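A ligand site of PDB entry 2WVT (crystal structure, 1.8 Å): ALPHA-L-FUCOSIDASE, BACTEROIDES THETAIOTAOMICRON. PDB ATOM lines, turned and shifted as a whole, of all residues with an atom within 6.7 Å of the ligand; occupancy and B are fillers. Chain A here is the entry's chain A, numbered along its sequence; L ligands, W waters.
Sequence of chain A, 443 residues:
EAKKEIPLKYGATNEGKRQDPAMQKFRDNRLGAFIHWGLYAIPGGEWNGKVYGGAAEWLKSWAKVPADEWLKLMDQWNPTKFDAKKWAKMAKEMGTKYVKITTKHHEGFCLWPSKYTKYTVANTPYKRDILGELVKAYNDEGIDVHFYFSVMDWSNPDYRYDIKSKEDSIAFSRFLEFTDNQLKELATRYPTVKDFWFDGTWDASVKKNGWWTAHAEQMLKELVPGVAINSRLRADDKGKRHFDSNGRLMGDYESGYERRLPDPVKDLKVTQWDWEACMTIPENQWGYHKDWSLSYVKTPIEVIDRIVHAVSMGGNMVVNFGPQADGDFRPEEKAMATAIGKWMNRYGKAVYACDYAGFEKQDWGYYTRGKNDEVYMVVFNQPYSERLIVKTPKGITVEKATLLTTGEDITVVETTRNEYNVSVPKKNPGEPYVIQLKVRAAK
The backbone NH of Gly 287 lies within hydrogen-bond range of the side-chain carboxylate of Glu 57, at 2.9 Å. The side-chain carboxylate (OD2) of Asp 199 sits at hydrogen-bond distance from the side-chain hydroxyl (OH) of Tyr 148 (2.8 Å). The guanidinium group (NH1) of Arg 232 lies within salt-bridge range of the side-chain carboxylate (OD1) of Asp 199. OE1 of Glu 258 is in salt-bridge range of NH2 of Arg 232. The backbone NH of Trp 286 lies within hydrogen-bond range of the side-chain carboxylate of Glu 57 (3.2 Å). The side-chain hydroxyl (OH) of Tyr 148 lies close to a ring nitrogen (NE2) of His 105.
A ring nitrogen (NE2) of His 105 sits at hydrogen-bond distance from an oxygen (O3) of the ligand (2.9 Å). O4 of the ligand is in hydrogen-bond range of SG of Cys 278 (3.6 Å). The side-chain carboxylate of Asp 199 is in salt-bridge range of a nitrogen (N1) of the ligand, at 2.7 Å. O1 of the ligand lies within hydrogen-bond range of NE2 of His 106, 2.8 Å away. An oxygen (O3) of the ligand is in hydrogen-bond range of a ring nitrogen (NE2) of His 36 (2.7 Å). NE1 of Trp 58 sits at hydrogen-bond distance from O1 of the ligand, at 2.8 Å. The side-chain carboxylate of Glu 258 is in salt-bridge range of a nitrogen (N1) of the ligand (3.5 Å). The side-chain carboxylate (OE2) of Glu 57 lies within hydrogen-bond range of an oxygen (O2) of the ligand.
Tyr 148 touches the ligand (OH to O3, 3.6 Å). Trp 197 touches the ligand. Trp 202 touches the ligand. Arg 232 touches the ligand. CZ2 of Trp 286 touches C5 of the ligand (3.6 Å). Hydrophobic or aromatic side chains within 4 Å of the ligand: His 36, Trp 58, His 105, His 106, Tyr 148, Trp 197, Trp 202 and Trp 286. Of the 20 residues printed, 13 come within 4 Å of the ligand.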
ATOM      1  N   PHE A  34     -22.367 -16.923 -14.245  1.00  0.00           N
ATOM      2  CA  PHE A  34     -22.568 -17.597 -15.517  1.00  0.00           C
ATOM      3  C   PHE A  34     -23.032 -16.504 -16.487  1.00  0.00           C
ATOM      4  O   PHE A  34     -23.835 -15.662 -16.117  1.00  0.00           O
ATOM      5  CB  PHE A  34     -23.665 -18.686 -15.395  1.00  0.00           C
ATOM      6  CG  PHE A  34     -23.254 -20.041 -15.931  1.00  0.00           C
ATOM      7  CD1 PHE A  34     -23.394 -21.175 -15.137  1.00  0.00           C
ATOM      8  CD2 PHE A  34     -22.711 -20.179 -17.202  1.00  0.00           C
ATOM      9  CE1 PHE A  34     -22.985 -22.447 -15.602  1.00  0.00           C
ATOM     10  CE2 PHE A  34     -22.300 -21.431 -17.674  1.00  0.00           C
ATOM     11  CZ  PHE A  34     -22.452 -22.566 -16.874  1.00  0.00           C
ATOM     12  N   HIS A  36     -24.848 -16.609 -20.122  1.00  0.00           N
ATOM     13  CA  HIS A  36     -25.425 -17.206 -21.331  1.00  0.00           C
ATOM     14  C   HIS A  36     -25.714 -16.055 -22.294  1.00  0.00           C
ATOM     15  O   HIS A  36     -26.699 -15.292 -22.113  1.00  0.00           O
ATOM     16  CB  HIS A  36     -26.720 -17.977 -21.052  1.00  0.00           C
ATOM     17  CG  HIS A  36     -26.516 -19.370 -20.521  1.00  0.00           C
ATOM     18  ND1 HIS A  36     -26.030 -19.618 -19.248  1.00  0.00           N
ATOM     19  CD2 HIS A  36     -26.783 -20.584 -21.067  1.00  0.00           C
ATOM     20  CE1 HIS A  36     -25.987 -20.924 -19.050  1.00  0.00           C
ATOM     21  NE2 HIS A  36     -26.458 -21.541 -20.123  1.00  0.00           N
ATOM     22  N   ALA A  55     -37.235 -22.023 -21.536  1.00  0.00           N
ATOM     23  CA  ALA A  55     -35.939 -21.338 -21.467  1.00  0.00           C
ATOM     24  C   ALA A  55     -35.643 -20.715 -22.819  1.00  0.00           C
ATOM     25  O   ALA A  55     -35.672 -21.408 -23.832  1.00  0.00           O
ATOM     26  CB  ALA A  55     -34.873 -22.292 -21.110  1.00  0.00           C
ATOM     27  N   GLU A  57     -33.002 -19.821 -24.308  1.00  0.00           N
ATOM     28  CA  GLU A  57     -31.862 -20.324 -25.084  1.00  0.00           C
ATOM     29  C   GLU A  57     -32.211 -21.608 -25.872  1.00  0.00           C
ATOM     30  O   GLU A  57     -31.451 -22.039 -26.744  1.00  0.00           O
ATOM     31  CB  GLU A  57     -30.606 -20.476 -24.220  1.00  0.00           C
ATOM     32  CG  GLU A  57     -30.578 -21.660 -23.255  1.00  0.00           C
ATOM     33  CD  GLU A  57     -31.471 -21.492 -22.034  1.00  0.00           C
ATOM     34  OE1 GLU A  57     -32.019 -20.380 -21.829  1.00  0.00           O
ATOM     35  OE2 GLU A  57     -31.575 -22.470 -21.263  1.00  0.00           O
ATOM     36  N   TRP A  58     -33.384 -22.172 -25.596  1.00  0.00           N
ATOM     37  CA  TRP A  58     -33.947 -23.329 -26.340  1.00  0.00           C
ATOM     38  C   TRP A  58     -35.069 -22.929 -27.314  1.00  0.00           C
ATOM     39  O   TRP A  58     -35.813 -23.817 -27.818  1.00  0.00           O
ATOM     40  CB  TRP A  58     -34.509 -24.349 -25.365  1.00  0.00           C
ATOM     41  CG  TRP A  58     -33.477 -25.243 -24.728  1.00  0.00           C
ATOM     42  CD1 TRP A  58     -32.651 -24.917 -23.707  1.00  0.00           C
ATOM     43  CD2 TRP A  58     -33.211 -26.616 -25.058  1.00  0.00           C
ATOM     44  NE1 TRP A  58     -31.856 -26.001 -23.382  1.00  0.00           N
ATOM     45  CE2 TRP A  58     -32.179 -27.049 -24.199  1.00  0.00           C
ATOM     46  CE3 TRP A  58     -33.726 -27.508 -26.009  1.00  0.00           C
ATOM     47  CZ2 TRP A  58     -31.651 -28.337 -24.262  1.00  0.00           C
ATOM     48  CZ3 TRP A  58     -33.223 -28.779 -26.056  1.00  0.00           C
ATOM     49  CH2 TRP A  58     -32.192 -29.192 -25.195  1.00  0.00           C
ATOM     50  N   THR A 102     -20.542 -18.827 -22.026  1.00  0.00           N
ATOM     51  CA  THR A 102     -20.909 -19.719 -23.121  1.00  0.00           C
ATOM     52  C   THR A 102     -20.088 -19.384 -24.369  1.00  0.00           C
ATOM     53  O   THR A 102     -20.412 -18.438 -25.104  1.00  0.00           O
ATOM     54  CB  THR A 102     -22.371 -19.557 -23.478  1.00  0.00           C
ATOM     55  OG1 THR A 102     -22.638 -18.162 -23.661  1.00  0.00           O
ATOM     56  CG2 THR A 102     -23.277 -20.121 -22.387  1.00  0.00           C
ATOM     57  N   HIS A 105     -23.282 -22.179 -27.289  1.00  0.00           N
ATOM     58  CA  HIS A 105     -24.347 -22.951 -26.700  1.00  0.00           C
ATOM     59  C   HIS A 105     -24.825 -23.995 -27.731  1.00  0.00           C
ATOM     60  O   HIS A 105     -24.151 -24.214 -28.741  1.00  0.00           O
ATOM     61  CB  HIS A 105     -25.472 -22.012 -26.237  1.00  0.00           C
ATOM     62  CG  HIS A 105     -26.318 -22.585 -25.139  1.00  0.00           C
ATOM     63  ND1 HIS A 105     -27.544 -23.169 -25.375  1.00  0.00           N
ATOM     64  CD2 HIS A 105     -26.104 -22.670 -23.803  1.00  0.00           C
ATOM     65  CE1 HIS A 105     -28.041 -23.600 -24.229  1.00  0.00           C
ATOM     66  NE2 HIS A 105     -27.186 -23.317 -23.267  1.00  0.00           N
ATOM     67  N   HIS A 106     -25.971 -24.656 -27.468  1.00  0.00           N
ATOM     68  CA  HIS A 106     -26.491 -25.683 -28.394  1.00  0.00           C
ATOM     69  C   HIS A 106     -26.682 -25.153 -29.830  1.00  0.00           C
ATOM     70  O   HIS A 106     -26.420 -25.868 -30.800  1.00  0.00           O
ATOM     71  CB  HIS A 106     -27.844 -26.266 -27.901  1.00  0.00           C
ATOM     72  CG  HIS A 106     -27.845 -26.695 -26.459  1.00  0.00           C
ATOM     73  ND1 HIS A 106     -26.730 -27.184 -25.802  1.00  0.00           N
ATOM     74  CD2 HIS A 106     -28.861 -26.722 -25.549  1.00  0.00           C
ATOM     75  CE1 HIS A 106     -27.057 -27.485 -24.570  1.00  0.00           C
ATOM     76  NE2 HIS A 106     -28.328 -27.219 -24.385  1.00  0.00           N
ATOM     77  N   TYR A 148     -17.717 -22.369 -20.870  1.00  0.00           N
ATOM     78  CA  TYR A 148     -18.804 -23.287 -21.134  1.00  0.00           C
ATOM     79  C   TYR A 148     -18.705 -23.675 -22.620  1.00  0.00           C
ATOM     80  O   TYR A 148     -18.507 -22.813 -23.490  1.00  0.00           O
ATOM     81  CB  TYR A 148     -20.127 -22.612 -20.834  1.00  0.00           C
ATOM     82  CG  TYR A 148     -21.334 -23.340 -21.333  1.00  0.00           C
ATOM     83  CD1 TYR A 148     -22.276 -23.886 -20.439  1.00  0.00           C
ATOM     84  CD2 TYR A 148     -21.574 -23.456 -22.679  1.00  0.00           C
ATOM     85  CE1 TYR A 148     -23.420 -24.534 -20.910  1.00  0.00           C
ATOM     86  CE2 TYR A 148     -22.705 -24.112 -23.158  1.00  0.00           C
ATOM     87  CZ  TYR A 148     -23.612 -24.645 -22.273  1.00  0.00           C
ATOM     88  OH  TYR A 148     -24.695 -25.284 -22.808  1.00  0.00           O
ATOM     89  N   MET A 152     -23.092 -30.995 -27.879  1.00  0.00           N
ATOM     90  CA  MET A 152     -24.281 -30.929 -28.754  1.00  0.00           C
ATOM     91  C   MET A 152     -24.317 -29.605 -29.526  1.00  0.00           C
ATOM     92  O   MET A 152     -24.238 -28.544 -28.939  1.00  0.00           O
ATOM     93  CB  MET A 152     -25.592 -31.088 -27.969  1.00  0.00           C
ATOM     94  CG  MET A 152     -26.841 -31.092 -28.880  1.00  0.00           C
ATOM     95  SD  MET A 152     -28.351 -31.621 -28.113  1.00  0.00           S
ATOM     96  CE  MET A 152     -28.598 -30.329 -26.872  1.00  0.00           C
ATOM     97  N   TRP A 197     -16.281 -26.301 -18.864  1.00  0.00           N
ATOM     98  CA  TRP A 197     -17.506 -26.815 -18.314  1.00  0.00           C
ATOM     99  C   TRP A 197     -18.333 -27.275 -19.498  1.00  0.00           C
ATOM    100  O   TRP A 197     -18.919 -26.473 -20.222  1.00  0.00           O
ATOM    101  CB  TRP A 197     -18.235 -25.752 -17.507  1.00  0.00           C
ATOM    102  CG  TRP A 197     -19.284 -26.277 -16.570  1.00  0.00           C
ATOM    103  CD1 TRP A 197     -19.116 -26.673 -15.273  1.00  0.00           C
ATOM    104  CD2 TRP A 197     -20.677 -26.451 -16.861  1.00  0.00           C
ATOM    105  NE1 TRP A 197     -20.321 -27.065 -14.724  1.00  0.00           N
ATOM    106  CE2 TRP A 197     -21.290 -26.932 -15.672  1.00  0.00           C
ATOM    107  CE3 TRP A 197     -21.458 -26.231 -17.985  1.00  0.00           C
ATOM    108  CZ2 TRP A 197     -22.640 -27.219 -15.617  1.00  0.00           C
ATOM    109  CZ3 TRP A 197     -22.802 -26.510 -17.916  1.00  0.00           C
ATOM    110  CH2 TRP A 197     -23.381 -26.988 -16.737  1.00  0.00           C
ATOM    111  N   ASP A 199     -21.332 -29.275 -21.543  1.00  0.00           N
ATOM    112  CA  ASP A 199     -22.771 -29.400 -21.443  1.00  0.00           C
ATOM    113  C   ASP A 199     -23.237 -30.098 -22.704  1.00  0.00           C
ATOM    114  O   ASP A 199     -22.436 -30.261 -23.616  1.00  0.00           O
ATOM    115  CB  ASP A 199     -23.405 -28.010 -21.348  1.00  0.00           C
ATOM    116  CG  ASP A 199     -24.784 -28.025 -20.724  1.00  0.00           C
ATOM    117  OD1 ASP A 199     -25.236 -29.083 -20.215  1.00  0.00           O
ATOM    118  OD2 ASP A 199     -25.431 -26.945 -20.742  1.00  0.00           O
ATOM    119  N   GLY A 200     -24.501 -30.529 -22.786  1.00  0.00           N
ATOM    120  CA  GLY A 200     -24.970 -31.167 -24.041  1.00  0.00           C
ATOM    121  C   GLY A 200     -24.183 -32.447 -24.372  1.00  0.00           C
ATOM    122  O   GLY A 200     -23.862 -32.718 -25.525  1.00  0.00           O
ATOM    123  N   TRP A 202     -25.323 -35.501 -22.839  1.00  0.00           N
ATOM    124  CA  TRP A 202     -26.249 -36.511 -22.319  1.00  0.00           C
ATOM    125  C   TRP A 202     -26.729 -37.522 -23.378  1.00  0.00           C
ATOM    126  O   TRP A 202     -27.346 -38.532 -23.018  1.00  0.00           O
ATOM    127  CB  TRP A 202     -27.491 -35.825 -21.699  1.00  0.00           C
ATOM    128  CG  TRP A 202     -28.133 -34.747 -22.598  1.00  0.00           C
ATOM    129  CD1 TRP A 202     -28.867 -34.937 -23.723  1.00  0.00           C
ATOM    130  CD2 TRP A 202     -28.069 -33.326 -22.394  1.00  0.00           C
ATOM    131  NE1 TRP A 202     -29.268 -33.724 -24.250  1.00  0.00           N
ATOM    132  CE2 TRP A 202     -28.794 -32.718 -23.446  1.00  0.00           C
ATOM    133  CE3 TRP A 202     -27.474 -32.511 -21.429  1.00  0.00           C
ATOM    134  CZ2 TRP A 202     -28.927 -31.324 -23.556  1.00  0.00           C
ATOM    135  CZ3 TRP A 202     -27.639 -31.099 -21.536  1.00  0.00           C
ATOM    136  CH2 TRP A 202     -28.359 -30.541 -22.602  1.00  0.00           C
ATOM    137  N   ARG A 232     -19.605 -33.511 -15.923  1.00  0.00           N
ATOM    138  CA  ARG A 232     -20.635 -33.595 -16.936  1.00  0.00           C
ATOM    139  C   ARG A 232     -20.119 -34.026 -18.311  1.00  0.00           C
ATOM    140  O   ARG A 232     -20.835 -34.663 -19.093  1.00  0.00           O
ATOM    141  CB  ARG A 232     -21.389 -32.262 -17.029  1.00  0.00           C
ATOM    142  CG  ARG A 232     -22.588 -32.298 -17.898  1.00  0.00           C
ATOM    143  CD  ARG A 232     -23.466 -31.048 -17.819  1.00  0.00           C
ATOM    144  NE  ARG A 232     -23.920 -30.661 -16.471  1.00  0.00           N
ATOM    145  CZ  ARG A 232     -25.054 -30.001 -16.242  1.00  0.00           C
ATOM    146  NH1 ARG A 232     -25.875 -29.695 -17.241  1.00  0.00           N
ATOM    147  NH2 ARG A 232     -25.380 -29.658 -15.009  1.00  0.00           N
ATOM    148  N   GLU A 258     -28.014 -28.359 -10.640  1.00  0.00           N
ATOM    149  CA  GLU A 258     -28.442 -27.330 -11.553  1.00  0.00           C
ATOM    150  C   GLU A 258     -29.845 -26.891 -11.147  1.00  0.00           C
ATOM    151  O   GLU A 258     -30.822 -27.623 -11.304  1.00  0.00           O
ATOM    152  CB  GLU A 258     -28.438 -27.932 -12.955  1.00  0.00           C
ATOM    153  CG  GLU A 258     -28.837 -27.032 -14.064  1.00  0.00           C
ATOM    154  CD  GLU A 258     -28.862 -27.783 -15.398  1.00  0.00           C
ATOM    155  OE1 GLU A 258     -28.137 -28.793 -15.538  1.00  0.00           O
ATOM    156  OE2 GLU A 258     -29.615 -27.366 -16.280  1.00  0.00           O
ATOM    157  N   CYS A 278     -24.965 -24.531 -10.228  1.00  0.00           N
ATOM    158  CA  CYS A 278     -25.382 -23.367 -10.976  1.00  0.00           C
ATOM    159  C   CYS A 278     -26.872 -23.110 -10.795  1.00  0.00           C
ATOM    160  O   CYS A 278     -27.633 -24.032 -10.479  1.00  0.00           O
ATOM    161  CB  CYS A 278     -25.047 -23.513 -12.458  1.00  0.00           C
ATOM    162  SG  CYS A 278     -25.669 -25.002 -13.236  1.00  0.00           S
ATOM    163  N   ASN A 284     -36.479 -20.962 -14.611  1.00  0.00           N
ATOM    164  CA  ASN A 284     -35.684 -21.659 -15.619  1.00  0.00           C
ATOM    165  C   ASN A 284     -35.492 -20.818 -16.882  1.00  0.00           C
ATOM    166  O   ASN A 284     -36.167 -21.038 -17.888  1.00  0.00           O
ATOM    167  CB  ASN A 284     -36.336 -23.002 -15.958  1.00  0.00           C
ATOM    168  CG  ASN A 284     -35.468 -23.889 -16.850  1.00  0.00           C
ATOM    169  OD1 ASN A 284     -34.398 -23.483 -17.301  1.00  0.00           O
ATOM    170  ND2 ASN A 284     -35.950 -25.099 -17.134  1.00  0.00           N
ATOM    171  N   TRP A 286     -31.891 -19.252 -18.814  1.00  0.00           N
ATOM    172  CA  TRP A 286     -30.462 -18.989 -18.785  1.00  0.00           C
ATOM    173  C   TRP A 286     -30.137 -17.841 -19.742  1.00  0.00           C
ATOM    174  O   TRP A 286     -29.550 -16.839 -19.345  1.00  0.00           O
ATOM    175  CB  TRP A 286     -29.682 -20.268 -19.128  1.00  0.00           C
ATOM    176  CG  TRP A 286     -29.956 -21.424 -18.167  1.00  0.00           C
ATOM    177  CD1 TRP A 286     -30.968 -22.355 -18.263  1.00  0.00           C
ATOM    178  CD2 TRP A 286     -29.207 -21.781 -16.996  1.00  0.00           C
ATOM    179  NE1 TRP A 286     -30.904 -23.253 -17.223  1.00  0.00           N
ATOM    180  CE2 TRP A 286     -29.834 -22.934 -16.424  1.00  0.00           C
ATOM    181  CE3 TRP A 286     -28.095 -21.233 -16.346  1.00  0.00           C
ATOM    182  CZ2 TRP A 286     -29.368 -23.543 -15.272  1.00  0.00           C
ATOM    183  CZ3 TRP A 286     -27.626 -21.851 -15.205  1.00  0.00           C
ATOM    184  CH2 TRP A 286     -28.264 -22.981 -14.665  1.00  0.00           C
ATOM    185  N   GLY A 287     -30.525 -17.982 -21.009  1.00  0.00           N
ATOM    186  CA  GLY A 287     -30.411 -16.874 -21.961  1.00  0.00           C
ATOM    187  C   GLY A 287     -31.446 -15.800 -21.697  1.00  0.00           C
ATOM    188  O   GLY A 287     -32.408 -16.009 -20.959  1.00  0.00           O
HETATM  189  O1  LIG L   1     -29.692 -27.101 -21.987  1.00  0.00           O
HETATM  190  C1  LIG L   1     -28.746 -26.444 -21.102  1.00  0.00           C
HETATM  191  C2  LIG L   1     -29.355 -25.144 -20.600  1.00  0.00           C
HETATM  192  O2  LIG L   1     -29.661 -24.349 -21.734  1.00  0.00           O
HETATM  193  C3  LIG L   1     -28.358 -24.445 -19.715  1.00  0.00           C
HETATM  194  O3  LIG L   1     -27.158 -24.115 -20.451  1.00  0.00           O
HETATM  195  C4  LIG L   1     -28.014 -25.371 -18.563  1.00  0.00           C
HETATM  196  C5  LIG L   1     -26.941 -24.728 -17.683  1.00  0.00           C
HETATM  197  O4  LIG L   1     -26.670 -25.637 -16.635  1.00  0.00           O
HETATM  198  N1  LIG L   1     -27.480 -26.693 -18.986  1.00  0.00           N
HETATM  199  C6  LIG L   1     -28.377 -27.358 -19.962  1.00  0.00           C
HETATM  200  C7  LIG L   1     -29.642 -27.948 -19.275  1.00  0.00           C
HETATM  201  O5  LIG L   1     -29.182 -28.761 -18.201  1.00  0.00           O
HETATM  202  O   HOH W   1     -29.080 -31.893 -18.321  1.00  0.00           O
